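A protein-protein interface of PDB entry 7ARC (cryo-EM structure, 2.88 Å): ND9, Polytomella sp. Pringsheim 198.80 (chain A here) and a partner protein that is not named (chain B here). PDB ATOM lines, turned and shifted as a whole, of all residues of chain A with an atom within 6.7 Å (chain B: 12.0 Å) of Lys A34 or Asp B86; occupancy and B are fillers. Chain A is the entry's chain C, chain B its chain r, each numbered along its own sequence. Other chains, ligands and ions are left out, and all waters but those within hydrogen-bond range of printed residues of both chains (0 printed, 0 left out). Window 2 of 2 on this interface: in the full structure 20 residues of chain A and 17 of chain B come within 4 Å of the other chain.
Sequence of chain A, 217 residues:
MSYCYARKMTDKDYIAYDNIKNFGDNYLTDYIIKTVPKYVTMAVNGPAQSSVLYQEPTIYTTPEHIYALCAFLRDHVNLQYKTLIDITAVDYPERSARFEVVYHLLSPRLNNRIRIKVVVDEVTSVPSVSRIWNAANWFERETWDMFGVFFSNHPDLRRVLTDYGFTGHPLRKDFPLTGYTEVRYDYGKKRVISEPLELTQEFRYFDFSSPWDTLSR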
ATOM      1  N   THR A  29      26.313 -23.356  31.875  1.00  0.00           N
ATOM      2  CA  THR A  29      26.745 -24.660  31.385  1.00  0.00           C
ATOM      3  C   THR A  29      27.506 -24.537  30.073  1.00  0.00           C
ATOM      4  O   THR A  29      28.544 -25.185  29.887  1.00  0.00           O
ATOM      5  CB  THR A  29      25.527 -25.564  31.216  1.00  0.00           C
ATOM      6  OG1 THR A  29      24.857 -25.703  32.474  1.00  0.00           O
ATOM      7  CG2 THR A  29      25.940 -26.920  30.732  1.00  0.00           C
ATOM      8  N   ASP A  30      27.005 -23.717  29.149  1.00  0.00           N
ATOM      9  CA  ASP A  30      27.697 -23.531  27.881  1.00  0.00           C
ATOM     10  C   ASP A  30      29.062 -22.900  28.110  1.00  0.00           C
ATOM     11  O   ASP A  30      30.051 -23.287  27.475  1.00  0.00           O
ATOM     12  CB  ASP A  30      26.855 -22.673  26.939  1.00  0.00           C
ATOM     13  CG  ASP A  30      25.406 -23.101  26.907  1.00  0.00           C
ATOM     14  OD1 ASP A  30      25.150 -24.323  26.846  1.00  0.00           O
ATOM     15  OD2 ASP A  30      24.519 -22.222  26.940  1.00  0.00           O
ATOM     16  N   TYR A  31      29.134 -21.933  29.026  1.00  0.00           N
ATOM     17  CA  TYR A  31      30.406 -21.303  29.352  1.00  0.00           C
ATOM     18  C   TYR A  31      31.400 -22.310  29.911  1.00  0.00           C
ATOM     19  O   TYR A  31      32.566 -22.325  29.506  1.00  0.00           O
ATOM     20  CB  TYR A  31      30.175 -20.182  30.362  1.00  0.00           C
ATOM     21  CG  TYR A  31      31.380 -19.321  30.649  1.00  0.00           C
ATOM     22  CD1 TYR A  31      31.903 -18.468  29.690  1.00  0.00           C
ATOM     23  CD2 TYR A  31      31.999 -19.371  31.884  1.00  0.00           C
ATOM     24  CE1 TYR A  31      33.005 -17.681  29.965  1.00  0.00           C
ATOM     25  CE2 TYR A  31      33.096 -18.594  32.164  1.00  0.00           C
ATOM     26  CZ  TYR A  31      33.595 -17.752  31.206  1.00  0.00           C
ATOM     27  OH  TYR A  31      34.690 -16.981  31.506  1.00  0.00           O
ATOM     28  N   ILE A  32      30.957 -23.177  30.824  1.00  0.00           N
ATOM     29  CA  ILE A  32      31.866 -24.173  31.388  1.00  0.00           C
ATOM     30  C   ILE A  32      32.352 -25.126  30.305  1.00  0.00           C
ATOM     31  O   ILE A  32      33.555 -25.387  30.178  1.00  0.00           O
ATOM     32  CB  ILE A  32      31.194 -24.931  32.545  1.00  0.00           C
ATOM     33  CG1 ILE A  32      31.061 -24.030  33.770  1.00  0.00           C
ATOM     34  CG2 ILE A  32      31.985 -26.179  32.895  1.00  0.00           C
ATOM     35  CD1 ILE A  32      29.908 -24.394  34.672  1.00  0.00           C
ATOM     36  N   ILE A  33      31.425 -25.658  29.505  1.00  0.00           N
ATOM     37  CA  ILE A  33      31.800 -26.630  28.479  1.00  0.00           C
ATOM     38  C   ILE A  33      32.783 -26.017  27.491  1.00  0.00           C
ATOM     39  O   ILE A  33      33.789 -26.634  27.126  1.00  0.00           O
ATOM     40  CB  ILE A  33      30.553 -27.182  27.769  1.00  0.00           C
ATOM     41  CG1 ILE A  33      29.801 -28.136  28.694  1.00  0.00           C
ATOM     42  CG2 ILE A  33      30.938 -27.889  26.484  1.00  0.00           C
ATOM     43  CD1 ILE A  33      28.330 -28.198  28.426  1.00  0.00           C
ATOM     44  N   LYS A  34      32.510 -24.792  27.042  1.00  0.00           N
ATOM     45  CA  LYS A  34      33.380 -24.160  26.059  1.00  0.00           C
ATOM     46  C   LYS A  34      34.738 -23.802  26.655  1.00  0.00           C
ATOM     47  O   LYS A  34      35.768 -23.960  25.990  1.00  0.00           O
ATOM     48  CB  LYS A  34      32.685 -22.939  25.464  1.00  0.00           C
ATOM     49  CG  LYS A  34      31.470 -23.325  24.631  1.00  0.00           C
ATOM     50  CD  LYS A  34      30.800 -22.129  23.992  1.00  0.00           C
ATOM     51  CE  LYS A  34      29.547 -22.543  23.240  1.00  0.00           C
ATOM     52  NZ  LYS A  34      29.854 -23.377  22.047  1.00  0.00           N
ATOM     53  N   THR A  35      34.765 -23.302  27.893  1.00  0.00           N
ATOM     54  CA  THR A  35      36.026 -22.874  28.492  1.00  0.00           C
ATOM     55  C   THR A  35      36.924 -24.062  28.816  1.00  0.00           C
ATOM     56  O   THR A  35      38.117 -24.054  28.493  1.00  0.00           O
ATOM     57  CB  THR A  35      35.751 -22.043  29.744  1.00  0.00           C
ATOM     58  OG1 THR A  35      34.829 -20.996  29.426  1.00  0.00           O
ATOM     59  CG2 THR A  35      37.032 -21.427  30.262  1.00  0.00           C
ATOM     60  N   VAL A  36      36.378 -25.094  29.453  1.00  0.00           N
ATOM     61  CA  VAL A  36      37.188 -26.240  29.864  1.00  0.00           C
ATOM     62  C   VAL A  36      36.585 -27.525  29.306  1.00  0.00           C
ATOM     63  O   VAL A  36      36.032 -28.341  30.056  1.00  0.00           O
ATOM     64  CB  VAL A  36      37.351 -26.288  31.393  1.00  0.00           C
ATOM     65  CG1 VAL A  36      38.238 -25.152  31.853  1.00  0.00           C
ATOM     66  CG2 VAL A  36      36.005 -26.171  32.089  1.00  0.00           C
ATOM     67  N   PRO A  37      36.692 -27.757  27.996  1.00  0.00           N
ATOM     68  CA  PRO A  37      35.989 -28.899  27.395  1.00  0.00           C
ATOM     69  C   PRO A  37      36.541 -30.256  27.798  1.00  0.00           C
ATOM     70  O   PRO A  37      35.760 -31.208  27.912  1.00  0.00           O
ATOM     71  CB  PRO A  37      36.139 -28.643  25.891  1.00  0.00           C
ATOM     72  CG  PRO A  37      37.375 -27.838  25.773  1.00  0.00           C
ATOM     73  CD  PRO A  37      37.452 -26.985  26.999  1.00  0.00           C
ATOM     74  N   VAL B  82      17.021 -32.727  25.220  1.00  0.00           N
ATOM     75  CA  VAL B  82      18.414 -33.087  24.977  1.00  0.00           C
ATOM     76  C   VAL B  82      19.034 -32.090  24.007  1.00  0.00           C
ATOM     77  O   VAL B  82      18.416 -31.720  23.004  1.00  0.00           O
ATOM     78  CB  VAL B  82      18.537 -34.523  24.422  1.00  0.00           C
ATOM     79  CG1 VAL B  82      19.981 -34.848  24.080  1.00  0.00           C
ATOM     80  CG2 VAL B  82      17.980 -35.528  25.412  1.00  0.00           C
ATOM     81  N   ARG B  83      20.257 -31.655  24.308  1.00  0.00           N
ATOM     82  CA  ARG B  83      21.051 -30.861  23.382  1.00  0.00           C
ATOM     83  C   ARG B  83      22.476 -31.396  23.349  1.00  0.00           C
ATOM     84  O   ARG B  83      22.915 -32.117  24.247  1.00  0.00           O
ATOM     85  CB  ARG B  83      21.091 -29.373  23.758  1.00  0.00           C
ATOM     86  CG  ARG B  83      19.778 -28.642  23.614  1.00  0.00           C
ATOM     87  CD  ARG B  83      19.948 -27.165  23.924  1.00  0.00           C
ATOM     88  NE  ARG B  83      20.230 -26.905  25.331  1.00  0.00           N
ATOM     89  CZ  ARG B  83      21.380 -26.427  25.785  1.00  0.00           C
ATOM     90  NH1 ARG B  83      22.394 -26.180  24.973  1.00  0.00           N
ATOM     91  NH2 ARG B  83      21.515 -26.190  27.087  1.00  0.00           N
ATOM     92  N   SER B  84      23.193 -31.037  22.289  1.00  0.00           N
ATOM     93  CA  SER B  84      24.605 -31.360  22.140  1.00  0.00           C
ATOM     94  C   SER B  84      25.387 -30.062  22.013  1.00  0.00           C
ATOM     95  O   SER B  84      25.035 -29.199  21.202  1.00  0.00           O
ATOM     96  CB  SER B  84      24.847 -32.255  20.922  1.00  0.00           C
ATOM     97  OG  SER B  84      26.226 -32.540  20.765  1.00  0.00           O
ATOM     98  N   VAL B  85      26.441 -29.923  22.811  1.00  0.00           N
ATOM     99  CA  VAL B  85      27.279 -28.731  22.812  1.00  0.00           C
ATOM    100  C   VAL B  85      28.657 -29.106  22.289  1.00  0.00           C
ATOM    101  O   VAL B  85      29.189 -30.173  22.618  1.00  0.00           O
ATOM    102  CB  VAL B  85      27.366 -28.104  24.218  1.00  0.00           C
ATOM    103  CG1 VAL B  85      28.202 -26.838  24.193  1.00  0.00           C
ATOM    104  CG2 VAL B  85      25.976 -27.792  24.731  1.00  0.00           C
ATOM    105  N   ASP B  86      29.230 -28.229  21.468  1.00  0.00           N
ATOM    106  CA  ASP B  86      30.522 -28.460  20.846  1.00  0.00           C
ATOM    107  C   ASP B  86      31.443 -27.279  21.103  1.00  0.00           C
ATOM    108  O   ASP B  86      30.995 -26.138  21.243  1.00  0.00           O
ATOM    109  CB  ASP B  86      30.384 -28.678  19.339  1.00  0.00           C
ATOM    110  CG  ASP B  86      29.815 -27.466  18.630  1.00  0.00           C
ATOM    111  OD1 ASP B  86      28.647 -27.114  18.896  1.00  0.00           O
ATOM    112  OD2 ASP B  86      30.538 -26.864  17.809  1.00  0.00           O
ATOM    113  N   SER B  87      32.742 -27.568  21.163  1.00  0.00           N
ATOM    114  CA  SER B  87      33.743 -26.540  21.413  1.00  0.00           C
ATOM    115  C   SER B  87      34.021 -25.675  20.189  1.00  0.00           C
ATOM    116  O   SER B  87      34.555 -24.572  20.339  1.00  0.00           O
ATOM    117  CB  SER B  87      35.042 -27.183  21.900  1.00  0.00           C
ATOM    118  OG  SER B  87      35.628 -27.977  20.885  1.00  0.00           O
ATOM    119  N   LYS B  88      33.682 -26.153  18.989  1.00  0.00           N
ATOM    120  CA  LYS B  88      34.002 -25.406  17.775  1.00  0.00           C
ATOM    121  C   LYS B  88      33.263 -24.074  17.727  1.00  0.00           C
ATOM    122  O   LYS B  88      33.846 -23.045  17.366  1.00  0.00           O
ATOM    123  CB  LYS B  88      33.659 -26.236  16.536  1.00  0.00           C
ATOM    124  CG  LYS B  88      34.714 -27.249  16.121  1.00  0.00           C
ATOM    125  CD  LYS B  88      34.737 -28.440  17.065  1.00  0.00           C
ATOM    126  CE  LYS B  88      33.474 -29.275  16.912  1.00  0.00           C
ATOM    127  NZ  LYS B  88      33.492 -30.486  17.778  1.00  0.00           N
ATOM    128  N   THR B  89      31.988 -24.071  18.081  1.00  0.00           N
ATOM    129  CA  THR B  89      31.202 -22.845  18.037  1.00  0.00           C
ATOM    130  C   THR B  89      31.625 -21.911  19.163  1.00  0.00           C
ATOM    131  O   THR B  89      31.609 -22.319  20.331  1.00  0.00           O
ATOM    132  CB  THR B  89      29.715 -23.164  18.147  1.00  0.00           C
ATOM    133  OG1 THR B  89      29.488 -24.000  19.288  1.00  0.00           O
ATOM    134  CG2 THR B  89      29.235 -23.888  16.899  1.00  0.00           C
ATOM    135  N   PRO B  90      32.013 -20.673  18.868  1.00  0.00           N
ATOM    136  CA  PRO B  90      32.477 -19.776  19.929  1.00  0.00           C
ATOM    137  C   PRO B  90      31.336 -19.337  20.831  1.00  0.00           C
ATOM    138  O   PRO B  90      30.178 -19.257  20.418  1.00  0.00           O
ATOM    139  CB  PRO B  90      33.065 -18.592  19.156  1.00  0.00           C
ATOM    140  CG  PRO B  90      32.296 -18.574  17.884  1.00  0.00           C
ATOM    141  CD  PRO B  90      32.028 -20.020  17.549  1.00  0.00           C
ATOM    142  N   PHE B  91      31.683 -19.053  22.082  1.00  0.00           N
ATOM    143  CA  PHE B  91      30.712 -18.531  23.030  1.00  0.00           C
ATOM    144  C   PHE B  91      30.392 -17.075  22.713  1.00  0.00           C
ATOM    145  O   PHE B  91      31.235 -16.323  22.218  1.00  0.00           O
ATOM    146  CB  PHE B  91      31.244 -18.660  24.457  1.00  0.00           C
ATOM    147  CG  PHE B  91      30.239 -18.327  25.519  1.00  0.00           C
ATOM    148  CD1 PHE B  91      29.104 -19.100  25.684  1.00  0.00           C
ATOM    149  CD2 PHE B  91      30.439 -17.251  26.366  1.00  0.00           C
ATOM    150  CE1 PHE B  91      28.183 -18.798  26.664  1.00  0.00           C
ATOM    151  CE2 PHE B  91      29.521 -16.946  27.348  1.00  0.00           C
ATOM    152  CZ  PHE B  91      28.392 -17.719  27.497  1.00  0.00           C
ATOM    153  N   ASP B  92      29.153 -16.683  22.999  1.00  0.00           N
ATOM    154  CA  ASP B  92      28.681 -15.323  22.744  1.00  0.00           C
ATOM    155  C   ASP B  92      28.940 -14.472  23.980  1.00  0.00           C
ATOM    156  O   ASP B  92      28.133 -14.425  24.909  1.00  0.00           O
ATOM    157  CB  ASP B  92      27.207 -15.327  22.367  1.00  0.00           C
ATOM    158  CG  ASP B  92      26.873 -14.293  21.311  1.00  0.00           C
ATOM    159  OD1 ASP B  92      27.768 -13.503  20.942  1.00  0.00           O
ATOM    160  OD2 ASP B  92      25.711 -14.265  20.853  1.00  0.00           O
ATOM    161  N   TYR B  93      30.088 -13.793  23.995  1.00  0.00           N
ATOM    162  CA  TYR B  93      30.395 -12.848  25.061  1.00  0.00           C
ATOM    163  C   TYR B  93      29.641 -11.537  24.918  1.00  0.00           C
ATOM    164  O   TYR B  93      29.596 -10.760  25.877  1.00  0.00           O
ATOM    165  CB  TYR B  93      31.899 -12.576  25.106  1.00  0.00           C
ATOM    166  CG  TYR B  93      32.705 -13.798  25.457  1.00  0.00           C
ATOM    167  CD1 TYR B  93      32.744 -14.275  26.758  1.00  0.00           C
ATOM    168  CD2 TYR B  93      33.411 -14.488  24.484  1.00  0.00           C
ATOM    169  CE1 TYR B  93      33.474 -15.398  27.082  1.00  0.00           C
ATOM    170  CE2 TYR B  93      34.143 -15.610  24.797  1.00  0.00           C
ATOM    171  CZ  TYR B  93      34.171 -16.062  26.097  1.00  0.00           C
ATOM    172  OH  TYR B  93      34.899 -17.184  26.411  1.00  0.00           O
ATOM    173  N   SER B  94      29.060 -11.270  23.747  1.00  0.00           N
ATOM    174  CA  SER B  94      28.202 -10.102  23.595  1.00  0.00           C
ATOM    175  C   SER B  94      26.990 -10.191  24.512  1.00  0.00           C
ATOM    176  O   SER B  94      26.570  -9.190  25.098  1.00  0.00           O
ATOM    177  CB  SER B  94      27.766  -9.952  22.138  1.00  0.00           C
ATOM    178  OG  SER B  94      28.877  -9.701  21.297  1.00  0.00           O
ATOM    179  N   LYS B  95      26.427 -11.390  24.664  1.00  0.00           N
ATOM    180  CA  LYS B  95      25.287 -11.565  25.558  1.00  0.00           C
ATOM    181  C   LYS B  95      25.664 -11.290  27.008  1.00  0.00           C
ATOM    182  O   LYS B  95      24.892 -10.676  27.753  1.00  0.00           O
ATOM    183  CB  LYS B  95      24.725 -12.977  25.405  1.00  0.00           C
ATOM    184  CG  LYS B  95      24.459 -13.377  23.964  1.00  0.00           C
ATOM    185  CD  LYS B  95      23.355 -12.535  23.345  1.00  0.00           C
ATOM    186  CE  LYS B  95      21.999 -12.887  23.931  1.00  0.00           C
ATOM    187  NZ  LYS B  95      21.357 -14.018  23.205  1.00  0.00           N
ATOM    188  N   VAL B  96      26.843 -11.748  27.433  1.00  0.00           N
ATOM    189  CA  VAL B  96      27.221 -11.647  28.839  1.00  0.00           C
ATOM    190  C   VAL B  96      27.532 -10.203  29.223  1.00  0.00           C
ATOM    191  O   VAL B  96      27.043  -9.698  30.240  1.00  0.00           O
ATOM    192  CB  VAL B  96      28.412 -12.576  29.139  1.00  0.00           C
ATOM    193  CG1 VAL B  96      28.913 -12.360  30.560  1.00  0.00           C
ATOM    194  CG2 VAL B  96      28.022 -14.028  28.919  1.00  0.00           C
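Of chain B, only Asp B86 (3.1 Å), Thr B89 (2.7 Å) and Phe B91 (3.5 Å) come within 4 Å of Lys A34. Ile A33 touches one residue of chain B. Thr A35 touches none of the printed residues of chain B. No residue of chain B comes within 4 Å of Val A36. No residue of chain B comes within 4 Å of Pro A37. Of the printed residues of chain A, Thr B89 touches Lys A34 (2.7 Å). Printed residues of chain A within 4 Å of Phe B91: Tyr A31 and Lys A34. Printed residues of chain A within 4 Å of Tyr B93: Tyr A31 (3.7 Å). Of the printed residues of chain A, Val B85 touches Ile A33 (3.7 Å). Of the printed residues of chain A, Arg B83 touches Asp A30. Ile A32 touches none of the printed residues of chain B. The nearest residue of chain B that does not touch Lys A34 is Pro B90 (4.3 Å). The nearest residue of chain A that does not touch Asp B86 is Ile A33 (5.3 Å).
CE2 of Phe B91 touches CD1 of Tyr A31 (3.7 Å). CE1 of Tyr B93 touches CE1 of Tyr A31 (3.7 Å). CG1 of Val B85 touches CG2 of Ile A33, at 3.7 Å. Phe B91 touches Lys A34 (CB to CD, 3.5 Å).
Of the 9 printed residues of chain A, 4 touch a printed residue of chain B. Hydrophobic or aromatic side chains of chain A that line the printed part of chain B: Tyr A31 and Ile A33. Printed residues of chain B that touch a printed residue of chain A: Arg B83, Val B85, Asp B86, Thr B89, Phe B91 and Tyr B93. Hydrophobic or aromatic side chains of chain B within 4 Å of the printed part of chain A: Val B85, Phe B91 and Tyr B93. Among the printed residues, Asp or Glu carboxylates within 4 Å of a Lys or Arg side-chain nitrogen of the other chain: Asp A30 with Arg B83 (3.8 Å).
NH1 of Arg B83 lies within salt-bridge range of OD1 of Asp A30, at 3.8 Å. O of Asp B86 sits at hydrogen-bond distance from NZ of Lys A34 (3.1 Å). O of Thr B89 is in hydrogen-bond range of NZ of Lys A34 (2.7 Å).
The backbone carbonyl oxygen (O) of Tyr A31 sits at hydrogen-bond distance from the side-chain hydroxyl (OG1) of Thr A35, 2.6 Å away. The side-chain carboxylate (OD2) of Asp B86 lies within hydrogen-bond range of the backbone NH (N) of Thr B89 (3.2 Å). N of Lys B88 lies close to OD2 of Asp B86 (3.4 Å).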
